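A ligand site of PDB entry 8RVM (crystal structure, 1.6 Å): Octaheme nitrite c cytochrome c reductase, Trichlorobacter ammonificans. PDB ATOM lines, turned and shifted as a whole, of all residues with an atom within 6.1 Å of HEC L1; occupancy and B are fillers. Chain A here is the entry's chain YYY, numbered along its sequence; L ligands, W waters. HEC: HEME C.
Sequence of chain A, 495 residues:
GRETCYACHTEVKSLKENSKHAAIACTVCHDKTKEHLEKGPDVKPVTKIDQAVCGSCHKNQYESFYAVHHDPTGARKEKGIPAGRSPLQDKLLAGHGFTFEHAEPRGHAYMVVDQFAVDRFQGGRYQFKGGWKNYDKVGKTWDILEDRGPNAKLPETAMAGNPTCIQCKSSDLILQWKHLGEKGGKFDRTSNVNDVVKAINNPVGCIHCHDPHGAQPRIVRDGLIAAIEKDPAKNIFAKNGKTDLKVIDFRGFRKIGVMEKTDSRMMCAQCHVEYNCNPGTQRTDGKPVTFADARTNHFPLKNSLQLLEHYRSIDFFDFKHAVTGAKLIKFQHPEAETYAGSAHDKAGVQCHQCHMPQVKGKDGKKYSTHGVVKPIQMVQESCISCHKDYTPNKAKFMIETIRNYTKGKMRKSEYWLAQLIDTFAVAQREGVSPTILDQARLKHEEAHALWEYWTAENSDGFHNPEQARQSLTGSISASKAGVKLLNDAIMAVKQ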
ATOM      1  N   GLY A   1     -14.189   6.069 -11.953  1.00  0.00           N
ATOM      2  CA  GLY A   1     -13.117   5.138 -11.406  1.00  0.00           C
ATOM      3  C   GLY A   1     -12.187   4.594 -12.485  1.00  0.00           C
ATOM      4  O   GLY A   1     -11.484   3.583 -12.205  1.00  0.00           O
ATOM      5  N   ARG A   2     -12.135   5.259 -13.651  1.00  0.00           N
ATOM      6  CA  ARG A   2     -11.268   4.884 -14.805  1.00  0.00           C
ATOM      7  C   ARG A   2      -9.812   4.646 -14.360  1.00  0.00           C
ATOM      8  O   ARG A   2      -9.139   3.765 -14.949  1.00  0.00           O
ATOM      9  CB  ARG A   2     -11.357   5.986 -15.877  1.00  0.00           C
ATOM     10  CG  ARG A   2     -10.811   7.318 -15.412  1.00  0.00           C
ATOM     11  CD  ARG A   2     -10.917   8.400 -16.466  1.00  0.00           C
ATOM     12  NE  ARG A   2     -12.298   8.690 -16.832  1.00  0.00           N
ATOM     13  CZ  ARG A   2     -12.655   9.362 -17.918  1.00  0.00           C
ATOM     14  NH1 ARG A   2     -11.739   9.827 -18.754  1.00  0.00           N
ATOM     15  NH2 ARG A   2     -13.933   9.570 -18.175  1.00  0.00           N
ATOM     16  N   THR A   4      -8.724   3.229 -11.735  1.00  0.00           N
ATOM     17  CA  THR A   4      -8.704   1.796 -11.339  1.00  0.00           C
ATOM     18  C   THR A   4      -8.373   0.934 -12.563  1.00  0.00           C
ATOM     19  O   THR A   4      -7.449   0.112 -12.484  1.00  0.00           O
ATOM     20  CB  THR A   4     -10.049   1.360 -10.761  1.00  0.00           C
ATOM     21  OG1 THR A   4     -10.341   2.245  -9.681  1.00  0.00           O
ATOM     22  CG2 THR A   4     -10.067  -0.068 -10.288  1.00  0.00           C
ATOM     23  N   CYS A   5      -9.155   1.101 -13.631  1.00  0.00           N
ATOM     24  CA  CYS A   5      -9.009   0.363 -14.916  1.00  0.00           C
ATOM     25  C   CYS A   5      -7.599   0.631 -15.476  1.00  0.00           C
ATOM     26  O   CYS A   5      -6.891  -0.337 -15.842  1.00  0.00           O
ATOM     27  CB  CYS A   5     -10.039   0.813 -15.951  1.00  0.00           C
ATOM     28  SG  CYS A   5     -11.718   0.924 -15.382  1.00  0.00           S
ATOM     29  N   TYR A   6      -7.244   1.914 -15.528  1.00  0.00           N
ATOM     30  CA  TYR A   6      -6.014   2.392 -16.223  1.00  0.00           C
ATOM     31  C   TYR A   6      -4.782   1.743 -15.598  1.00  0.00           C
ATOM     32  O   TYR A   6      -3.748   1.629 -16.292  1.00  0.00           O
ATOM     33  CB  TYR A   6      -5.927   3.910 -16.134  1.00  0.00           C
ATOM     34  CG  TYR A   6      -6.846   4.676 -17.038  1.00  0.00           C
ATOM     35  CD1 TYR A   6      -7.325   4.145 -18.233  1.00  0.00           C
ATOM     36  CD2 TYR A   6      -7.183   5.987 -16.744  1.00  0.00           C
ATOM     37  CE1 TYR A   6      -8.145   4.881 -19.068  1.00  0.00           C
ATOM     38  CE2 TYR A   6      -8.011   6.724 -17.563  1.00  0.00           C
ATOM     39  CZ  TYR A   6      -8.503   6.173 -18.731  1.00  0.00           C
ATOM     40  OH  TYR A   6      -9.311   6.892 -19.539  1.00  0.00           O
ATOM     41  N   ALA A   7      -4.879   1.321 -14.327  1.00  0.00           N
ATOM     42  CA  ALA A   7      -3.796   0.644 -13.592  1.00  0.00           C
ATOM     43  C   ALA A   7      -3.283  -0.552 -14.388  1.00  0.00           C
ATOM     44  O   ALA A   7      -2.055  -0.756 -14.387  1.00  0.00           O
ATOM     45  CB  ALA A   7      -4.278   0.211 -12.221  1.00  0.00           C
ATOM     46  N   CYS A   8      -4.157  -1.350 -15.024  1.00  0.00           N
ATOM     47  CA  CYS A   8      -3.735  -2.583 -15.753  1.00  0.00           C
ATOM     48  C   CYS A   8      -3.996  -2.437 -17.259  1.00  0.00           C
ATOM     49  O   CYS A   8      -3.759  -3.426 -17.979  1.00  0.00           O
ATOM     50  CB  CYS A   8      -4.432  -3.831 -15.233  1.00  0.00           C
ATOM     51  SG  CYS A   8      -4.747  -3.838 -13.466  1.00  0.00           S
ATOM     52  N   HIS A   9      -4.510  -1.296 -17.705  1.00  0.00           N
ATOM     53  CA  HIS A   9      -4.834  -1.019 -19.142  1.00  0.00           C
ATOM     54  C   HIS A   9      -4.258   0.333 -19.554  1.00  0.00           C
ATOM     55  O   HIS A   9      -5.018   1.344 -19.713  1.00  0.00           O
ATOM     56  CB  HIS A   9      -6.334  -1.113 -19.379  1.00  0.00           C
ATOM     57  CG  HIS A   9      -6.923  -2.455 -19.039  1.00  0.00           C
ATOM     58  ND1 HIS A   9      -6.503  -3.625 -19.624  1.00  0.00           N
ATOM     59  CD2 HIS A   9      -7.927  -2.785 -18.177  1.00  0.00           C
ATOM     60  CE1 HIS A   9      -7.222  -4.634 -19.137  1.00  0.00           C
ATOM     61  NE2 HIS A   9      -8.118  -4.136 -18.252  1.00  0.00           N
ATOM     62  N   CYS A  26     -16.566   4.417 -19.144  1.00  0.00           N
ATOM     63  CA  CYS A  26     -16.198   3.061 -19.640  1.00  0.00           C
ATOM     64  C   CYS A  26     -17.449   2.189 -19.813  1.00  0.00           C
ATOM     65  O   CYS A  26     -17.436   1.273 -20.680  1.00  0.00           O
ATOM     66  CB  CYS A  26     -15.287   2.337 -18.671  1.00  0.00           C
ATOM     67  SG  CYS A  26     -13.798   3.189 -18.218  1.00  0.00           S
ATOM     68  N   HIS A  30     -18.718  -0.901 -22.291  1.00  0.00           N
ATOM     69  CA  HIS A  30     -18.277  -2.154 -21.634  1.00  0.00           C
ATOM     70  C   HIS A  30     -19.282  -2.472 -20.510  1.00  0.00           C
ATOM     71  O   HIS A  30     -19.599  -1.565 -19.720  1.00  0.00           O
ATOM     72  CB  HIS A  30     -16.848  -2.045 -21.097  1.00  0.00           C
ATOM     73  CG  HIS A  30     -15.798  -1.778 -22.125  1.00  0.00           C
ATOM     74  ND1 HIS A  30     -15.267  -2.770 -22.900  1.00  0.00           N
ATOM     75  CD2 HIS A  30     -15.112  -0.652 -22.436  1.00  0.00           C
ATOM     76  CE1 HIS A  30     -14.317  -2.261 -23.671  1.00  0.00           C
ATOM     77  NE2 HIS A  30     -14.212  -0.964 -23.396  1.00  0.00           N
ATOM     78  N   THR A  33     -18.366  -4.610 -15.831  1.00  0.00           N
ATOM     79  CA  THR A  33     -17.099  -4.016 -15.342  1.00  0.00           C
ATOM     80  C   THR A  33     -17.002  -4.330 -13.834  1.00  0.00           C
ATOM     81  O   THR A  33     -15.923  -4.786 -13.439  1.00  0.00           O
ATOM     82  CB  THR A  33     -16.997  -2.545 -15.764  1.00  0.00           C
ATOM     83  OG1 THR A  33     -18.065  -1.823 -15.152  1.00  0.00           O
ATOM     84  CG2 THR A  33     -17.037  -2.391 -17.284  1.00  0.00           C
ATOM     85  N   LYS A  34     -18.068  -4.133 -13.058  1.00  0.00           N
ATOM     86  CA  LYS A  34     -18.069  -4.437 -11.600  1.00  0.00           C
ATOM     87  C   LYS A  34     -17.596  -5.883 -11.411  1.00  0.00           C
ATOM     88  O   LYS A  34     -16.622  -6.083 -10.685  1.00  0.00           O
ATOM     89  CB  LYS A  34     -19.437  -4.190 -10.944  1.00  0.00           C
ATOM     90  CG  LYS A  34     -19.931  -2.743 -10.962  1.00  0.00           C
ATOM     91  CD  LYS A  34     -18.938  -1.698 -10.489  1.00  0.00           C
ATOM     92  CE  LYS A  34     -18.267  -2.079  -9.178  1.00  0.00           C
ATOM     93  NZ  LYS A  34     -17.742  -0.912  -8.423  1.00  0.00           N
ATOM     94  N   HIS A  36     -15.783  -7.646 -13.301  1.00  0.00           N
ATOM     95  CA  HIS A  36     -14.354  -7.670 -13.684  1.00  0.00           C
ATOM     96  C   HIS A  36     -13.500  -7.126 -12.551  1.00  0.00           C
ATOM     97  O   HIS A  36     -12.416  -7.660 -12.347  1.00  0.00           O
ATOM     98  CB  HIS A  36     -14.163  -6.854 -14.967  1.00  0.00           C
ATOM     99  CG  HIS A  36     -12.791  -6.866 -15.546  1.00  0.00           C
ATOM    100  ND1 HIS A  36     -12.093  -8.034 -15.846  1.00  0.00           N
ATOM    101  CD2 HIS A  36     -12.001  -5.841 -15.966  1.00  0.00           C
ATOM    102  CE1 HIS A  36     -10.932  -7.711 -16.429  1.00  0.00           C
ATOM    103  NE2 HIS A  36     -10.834  -6.365 -16.510  1.00  0.00           N
ATOM    104  N   LEU A  37     -13.955  -6.066 -11.878  1.00  0.00           N
ATOM    105  CA  LEU A  37     -13.233  -5.479 -10.716  1.00  0.00           C
ATOM    106  C   LEU A  37     -13.303  -6.464  -9.537  1.00  0.00           C
ATOM    107  O   LEU A  37     -12.213  -6.873  -9.029  1.00  0.00           O
ATOM    108  CB  LEU A  37     -13.876  -4.135 -10.336  1.00  0.00           C
ATOM    109  CG  LEU A  37     -13.510  -2.958 -11.234  1.00  0.00           C
ATOM    110  CD1 LEU A  37     -14.040  -1.648 -10.667  1.00  0.00           C
ATOM    111  CD2 LEU A  37     -12.000  -2.875 -11.422  1.00  0.00           C
ATOM    112  N   PRO A  41      -9.496 -10.480 -13.142  1.00  0.00           N
ATOM    113  CA  PRO A  41      -9.339 -10.474 -14.587  1.00  0.00           C
ATOM    114  C   PRO A  41      -9.907 -11.706 -15.314  1.00  0.00           C
ATOM    115  O   PRO A  41     -10.130 -11.598 -16.503  1.00  0.00           O
ATOM    116  CB  PRO A  41      -7.817 -10.385 -14.770  1.00  0.00           C
ATOM    117  CG  PRO A  41      -7.266 -11.097 -13.541  1.00  0.00           C
ATOM    118  CD  PRO A  41      -8.224 -10.707 -12.440  1.00  0.00           C
ATOM    119  N   LYS A  44     -13.960 -11.378 -17.828  1.00  0.00           N
ATOM    120  CA  LYS A  44     -13.812 -10.300 -18.847  1.00  0.00           C
ATOM    121  C   LYS A  44     -15.080  -9.453 -18.878  1.00  0.00           C
ATOM    122  O   LYS A  44     -16.177 -10.008 -18.828  1.00  0.00           O
ATOM    123  CB  LYS A  44     -13.679 -10.913 -20.236  1.00  0.00           C
ATOM    124  CG  LYS A  44     -12.369 -11.620 -20.555  1.00  0.00           C
ATOM    125  CD  LYS A  44     -12.483 -12.511 -21.784  1.00  0.00           C
ATOM    126  CE  LYS A  44     -11.477 -12.186 -22.864  1.00  0.00           C
ATOM    127  NZ  LYS A  44     -10.083 -12.293 -22.374  1.00  0.00           N
ATOM    128  N   PRO A  45     -14.995  -8.111 -18.997  1.00  0.00           N
ATOM    129  CA  PRO A  45     -16.174  -7.310 -19.284  1.00  0.00           C
ATOM    130  C   PRO A  45     -16.743  -7.754 -20.638  1.00  0.00           C
ATOM    131  O   PRO A  45     -16.052  -8.414 -21.362  1.00  0.00           O
ATOM    132  CB  PRO A  45     -15.672  -5.871 -19.364  1.00  0.00           C
ATOM    133  CG  PRO A  45     -14.337  -5.908 -18.632  1.00  0.00           C
ATOM    134  CD  PRO A  45     -13.778  -7.297 -18.914  1.00  0.00           C
ATOM    135  N   VAL A  46     -17.978  -7.381 -20.925  1.00  0.00           N
ATOM    136  CA  VAL A  46     -18.567  -7.614 -22.271  1.00  0.00           C
ATOM    137  C   VAL A  46     -18.314  -6.327 -23.064  1.00  0.00           C
ATOM    138  O   VAL A  46     -18.579  -5.224 -22.533  1.00  0.00           O
ATOM    139  CB  VAL A  46     -20.058  -7.971 -22.210  1.00  0.00           C
ATOM    140  CG1 VAL A  46     -20.668  -8.042 -23.609  1.00  0.00           C
ATOM    141  CG2 VAL A  46     -20.267  -9.271 -21.464  1.00  0.00           C
ATOM    142  N   THR A  47     -17.788  -6.483 -24.265  1.00  0.00           N
ATOM    143  CA  THR A  47     -17.544  -5.357 -25.193  1.00  0.00           C
ATOM    144  C   THR A  47     -18.449  -5.577 -26.393  1.00  0.00           C
ATOM    145  O   THR A  47     -18.041  -6.334 -27.251  1.00  0.00           O
ATOM    146  CB  THR A  47     -16.068  -5.309 -25.583  1.00  0.00           C
ATOM    147  OG1 THR A  47     -15.291  -5.233 -24.386  1.00  0.00           O
ATOM    148  CG2 THR A  47     -15.771  -4.143 -26.502  1.00  0.00           C
ATOM    149  N   LEU A 175     -11.857  -8.418 -30.870  1.00  0.00           N
ATOM    150  CA  LEU A 175     -11.287  -8.990 -29.614  1.00  0.00           C
ATOM    151  C   LEU A 175     -11.237 -10.523 -29.642  1.00  0.00           C
ATOM    152  O   LEU A 175     -10.880 -11.109 -28.582  1.00  0.00           O
ATOM    153  CB  LEU A 175     -12.072  -8.521 -28.382  1.00  0.00           C
ATOM    154  CG  LEU A 175     -12.196  -7.000 -28.203  1.00  0.00           C
ATOM    155  CD1 LEU A 175     -13.109  -6.675 -27.030  1.00  0.00           C
ATOM    156  CD2 LEU A 175     -10.824  -6.355 -28.026  1.00  0.00           C
ATOM    157  N   ARG A 251      -1.199  -6.922 -25.609  1.00  0.00           N
ATOM    158  CA  ARG A 251      -0.948  -8.244 -24.984  1.00  0.00           C
ATOM    159  C   ARG A 251      -0.198  -9.183 -25.938  1.00  0.00           C
ATOM    160  O   ARG A 251      -0.205 -10.374 -25.674  1.00  0.00           O
ATOM    161  CB  ARG A 251      -2.284  -8.859 -24.564  1.00  0.00           C
ATOM    162  CG  ARG A 251      -3.177  -7.888 -23.805  1.00  0.00           C
ATOM    163  CD  ARG A 251      -4.558  -8.443 -23.560  1.00  0.00           C
ATOM    164  NE  ARG A 251      -5.491  -8.116 -24.636  1.00  0.00           N
ATOM    165  CZ  ARG A 251      -6.022  -8.973 -25.506  1.00  0.00           C
ATOM    166  NH1 ARG A 251      -5.697 -10.257 -25.472  1.00  0.00           N
ATOM    167  NH2 ARG A 251      -6.863  -8.534 -26.415  1.00  0.00           N
HETATM  168 FE   HEC L   1      -9.589  -5.086 -17.373  1.00  0.00          FE
HETATM  169  CHA HEC L   1      -9.495  -7.636 -19.679  1.00  0.00           C
HETATM  170  CHB HEC L   1     -11.838  -3.399 -19.268  1.00  0.00           C
HETATM  171  CHC HEC L   1     -10.088  -2.955 -14.666  1.00  0.00           C
HETATM  172  CHD HEC L   1      -6.851  -6.366 -15.845  1.00  0.00           C
HETATM  173  NA  HEC L   1     -10.489  -5.471 -19.205  1.00  0.00           N
HETATM  174  C1A HEC L   1     -10.340  -6.538 -19.989  1.00  0.00           C
HETATM  175  C2A HEC L   1     -11.121  -6.562 -21.225  1.00  0.00           C
HETATM  176  C3A HEC L   1     -11.844  -5.295 -21.105  1.00  0.00           C
HETATM  177  C4A HEC L   1     -11.361  -4.679 -19.837  1.00  0.00           C
HETATM  178  CMA HEC L   1     -12.813  -4.692 -22.056  1.00  0.00           C
HETATM  179  CAA HEC L   1     -11.215  -7.702 -22.227  1.00  0.00           C
HETATM  180  CBA HEC L   1     -10.564  -7.597 -23.583  1.00  0.00           C
HETATM  181  CGA HEC L   1     -10.961  -8.856 -24.347  1.00  0.00           C
HETATM  182  O1A HEC L   1     -10.106  -9.720 -24.622  1.00  0.00           O
HETATM  183  O2A HEC L   1     -12.163  -9.011 -24.646  1.00  0.00           O
HETATM  184  NB  HEC L   1     -10.735  -3.446 -17.017  1.00  0.00           N
HETATM  185  C1B HEC L   1     -11.581  -2.877 -17.911  1.00  0.00           C
HETATM  186  C2B HEC L   1     -12.290  -1.731 -17.403  1.00  0.00           C
HETATM  187  C3B HEC L   1     -11.753  -1.655 -16.033  1.00  0.00           C
HETATM  188  C4B HEC L   1     -10.860  -2.745 -15.906  1.00  0.00           C
HETATM  189  CMB HEC L   1     -13.310  -0.915 -18.135  1.00  0.00           C
HETATM  190  CAB HEC L   1     -12.086  -0.712 -14.970  1.00  0.00           C
HETATM  191  CBB HEC L   1     -13.535  -0.901 -14.564  1.00  0.00           C
HETATM  192  NC  HEC L   1      -8.661  -4.741 -15.526  1.00  0.00           N
HETATM  193  C1C HEC L   1      -8.984  -3.856 -14.577  1.00  0.00           C
HETATM  194  C2C HEC L   1      -8.051  -3.804 -13.442  1.00  0.00           C
HETATM  195  C3C HEC L   1      -7.122  -4.850 -13.829  1.00  0.00           C
HETATM  196  C4C HEC L   1      -7.546  -5.340 -15.129  1.00  0.00           C
HETATM  197  CMC HEC L   1      -8.120  -2.927 -12.219  1.00  0.00           C
HETATM  198  CAC HEC L   1      -5.872  -5.217 -13.130  1.00  0.00           C
HETATM  199  CBC HEC L   1      -5.987  -5.667 -11.705  1.00  0.00           C
HETATM  200  ND  HEC L   1      -8.466  -6.629 -17.696  1.00  0.00           N
HETATM  201  C1D HEC L   1      -7.355  -7.037 -17.017  1.00  0.00           C
HETATM  202  C2D HEC L   1      -6.681  -8.264 -17.447  1.00  0.00           C
HETATM  203  C3D HEC L   1      -7.494  -8.629 -18.586  1.00  0.00           C
HETATM  204  C4D HEC L   1      -8.526  -7.590 -18.597  1.00  0.00           C
HETATM  205  CMD HEC L   1      -5.452  -8.954 -16.904  1.00  0.00           C
HETATM  206  CAD HEC L   1      -7.436  -9.757 -19.566  1.00  0.00           C
HETATM  207  CBD HEC L   1      -6.249 -10.699 -19.581  1.00  0.00           C
HETATM  208  CGD HEC L   1      -6.436 -11.499 -20.865  1.00  0.00           C
HETATM  209  O1D HEC L   1      -5.634 -11.386 -21.812  1.00  0.00           O
HETATM  210  O2D HEC L   1      -7.443 -12.253 -20.950  1.00  0.00           O
HETATM  211 FE   HEC L   2     -12.960   0.278 -24.222  1.00  0.00          FE
HETATM  212  CHA HEC L   2     -11.563  -2.436 -26.041  1.00  0.00           C
HETATM  213  CHB HEC L   2     -10.956  -0.504 -21.599  1.00  0.00           C
HETATM  214  CHC HEC L   2     -14.043   3.152 -22.542  1.00  0.00           C
HETATM  215  CHD HEC L   2     -15.165   0.740 -26.690  1.00  0.00           C
HETATM  216  NA  HEC L   2     -11.653  -1.151 -23.984  1.00  0.00           N
HETATM  217  C1A HEC L   2     -11.128  -2.165 -24.689  1.00  0.00           C
HETATM  218  C2A HEC L   2     -10.110  -2.979 -24.080  1.00  0.00           C
HETATM  219  C3A HEC L   2      -9.944  -2.449 -22.789  1.00  0.00           C
HETATM  220  C4A HEC L   2     -10.897  -1.329 -22.812  1.00  0.00           C
HETATM  221  CMA HEC L   2      -8.965  -2.990 -21.792  1.00  0.00           C
HETATM  222  CAA HEC L   2      -9.376  -4.136 -24.615  1.00  0.00           C
HETATM  223  CBA HEC L   2      -7.977  -3.767 -25.103  1.00  0.00           C
HETATM  224  CGA HEC L   2      -7.099  -4.958 -25.228  1.00  0.00           C
HETATM  225  O1A HEC L   2      -7.015  -5.682 -26.319  1.00  0.00           O
HETATM  226  O2A HEC L   2      -6.384  -5.221 -24.213  1.00  0.00           O
HETATM  227  NB  HEC L   2     -12.559   1.173 -22.406  1.00  0.00           N
HETATM  228  C1B HEC L   2     -11.728   0.699 -21.461  1.00  0.00           C
HETATM  229  C2B HEC L   2     -11.653   1.517 -20.240  1.00  0.00           C
HETATM  230  C3B HEC L   2     -12.583   2.586 -20.519  1.00  0.00           C
HETATM  231  C4B HEC L   2     -13.098   2.284 -21.889  1.00  0.00           C
HETATM  232  CMB HEC L   2     -10.812   1.246 -19.020  1.00  0.00           C
HETATM  233  CAB HEC L   2     -12.939   3.743 -19.663  1.00  0.00           C
HETATM  234  CBB HEC L   2     -11.761   4.610 -19.294  1.00  0.00           C
HETATM  235  NC  HEC L   2     -14.331   1.726 -24.538  1.00  0.00           N
HETATM  236  C1C HEC L   2     -14.665   2.795 -23.826  1.00  0.00           C
HETATM  237  C2C HEC L   2     -15.726   3.587 -24.357  1.00  0.00           C
HETATM  238  C3C HEC L   2     -16.034   2.864 -25.616  1.00  0.00           C
HETATM  239  C4C HEC L   2     -15.162   1.736 -25.607  1.00  0.00           C
HETATM  240  CMC HEC L   2     -16.305   4.804 -23.763  1.00  0.00           C
HETATM  241  CAC HEC L   2     -17.119   3.171 -26.579  1.00  0.00           C
HETATM  242  CBC HEC L   2     -17.101   4.543 -27.126  1.00  0.00           C
HETATM  243  ND  HEC L   2     -13.300  -0.676 -26.042  1.00  0.00           N
HETATM  244  C1D HEC L   2     -14.272  -0.367 -26.872  1.00  0.00           C
HETATM  245  C2D HEC L   2     -14.265  -1.149 -28.087  1.00  0.00           C
HETATM  246  C3D HEC L   2     -13.205  -2.115 -27.912  1.00  0.00           C
HETATM  247  C4D HEC L   2     -12.679  -1.707 -26.595  1.00  0.00           C
HETATM  248  CMD HEC L   2     -15.264  -1.011 -29.202  1.00  0.00           C
HETATM  249  CAD HEC L   2     -12.673  -3.235 -28.767  1.00  0.00           C
HETATM  250  CBD HEC L   2     -11.255  -2.975 -29.355  1.00  0.00           C
HETATM  251  CGD HEC L   2     -11.008  -1.652 -30.096  1.00  0.00           C
HETATM  252  O1D HEC L   2      -9.832  -1.125 -30.053  1.00  0.00           O
HETATM  253  O2D HEC L   2     -11.984  -1.123 -30.710  1.00  0.00           O
HETATM  254  O   HOH W   1      -2.649  -7.800 -15.629  1.00  0.00           O
HETATM  255  O   HOH W   2      -7.021  -6.694 -21.952  1.00  0.00           O
HETATM  256  O   HOH W   3      -8.921 -10.568 -26.954  1.00  0.00           O
HETATM  257  O   HOH W   4     -14.517  -7.725 -23.992  1.00  0.00           O
HETATM  258  O   HOH W   5      -8.094  -9.269 -22.826  1.00  0.00           O
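Water W5 bridges an oxygen (O1A) of HEC L1 (2.7 Å) and the guanidinium group of Arg 251 (3.4 Å).
Water W3 lies within hydrogen-bond range of O of Leu 175 (2.6 Å), O1A of HEC L1 (2.7 Å) and NH2 of Arg 251 (2.9 Å).
Water W4 lies within hydrogen-bond range of OG1 of Thr 47, O2A of HEC L1 and O of Pro 45.
Water W2 bridges O2A of HEC L2 (2.8 Å) and NE of Arg 251 (3.4 Å).
A ring nitrogen (ND1) of His 30 sits at hydrogen-bond distance from the side-chain hydroxyl (OG1) of Thr 47.
O of Gly 1 lies close to OG1 of Thr 4.
O of Thr 4 touches CMC of HEC L1, at 3.1 Å.
Cys 26 touches HEC L1 (CB to CMB, 3.8 Å).
ND1 of His 30 touches CMA of HEC L1, at 3.2 Å.
Leu 37 touches HEC L1 (CD2 to CHC, 3.8 Å).
Pro 41 touches HEC L1.
CG of Pro 45 touches C4A of HEC L1, 3.4 Å away.
Thr 47 touches HEC L1 (OG1 to CMA, 3.4 Å).
Leu 175 touches HEC L1 (CD1 to O2A, 3.5 Å).
Hydrophobic or aromatic side chains that line HEC L1: His 9, His 30, His 36, Leu 37, Pro 41, Pro 45 and Leu 175.
Within 4 Å of HEC L1: Thr 4, Cys 5, Cys 8, His 9, Cys 26, His 30, His 36, Leu 37, Pro 41, Lys 44, Pro 45, Thr 47, Leu 175 and Arg 251.
The nearest printed residue that does not touch HEC L1 is Thr 33 (4.02 Å).
A ring nitrogen (NE2) of His 36 is bound to an iron atom (FE) of HEC L1, 2.0 Å away.
The side-chain amino group of Lys 44 lies within salt-bridge range of an oxygen (O2D) of HEC L1 (3.0 Å).
The side-chain sulfur of Cys 5 is covalently linked to a carbon (CAB) of HEC L1 (1.7 Å).
A ring nitrogen (NE2) of His 30 binds an iron atom (FE) of HEC L2, 1.9 Å away.
The side-chain sulfur (SG) of Cys 26 is covalently linked to a carbon (CAB) of HEC L2, at 1.8 Å.
NH2 of Arg 251 is in salt-bridge range of O1A of HEC L2 (2.9 Å).
CAC of HEC L1 is bonded to SG of Cys 8 (1.8 Å).
NE2 of His 9 binds FE of HEC L1, at 2.0 Å.
O1D of HEC L1 is in salt-bridge range of NH1 of Arg 251, at 3.8 Å.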
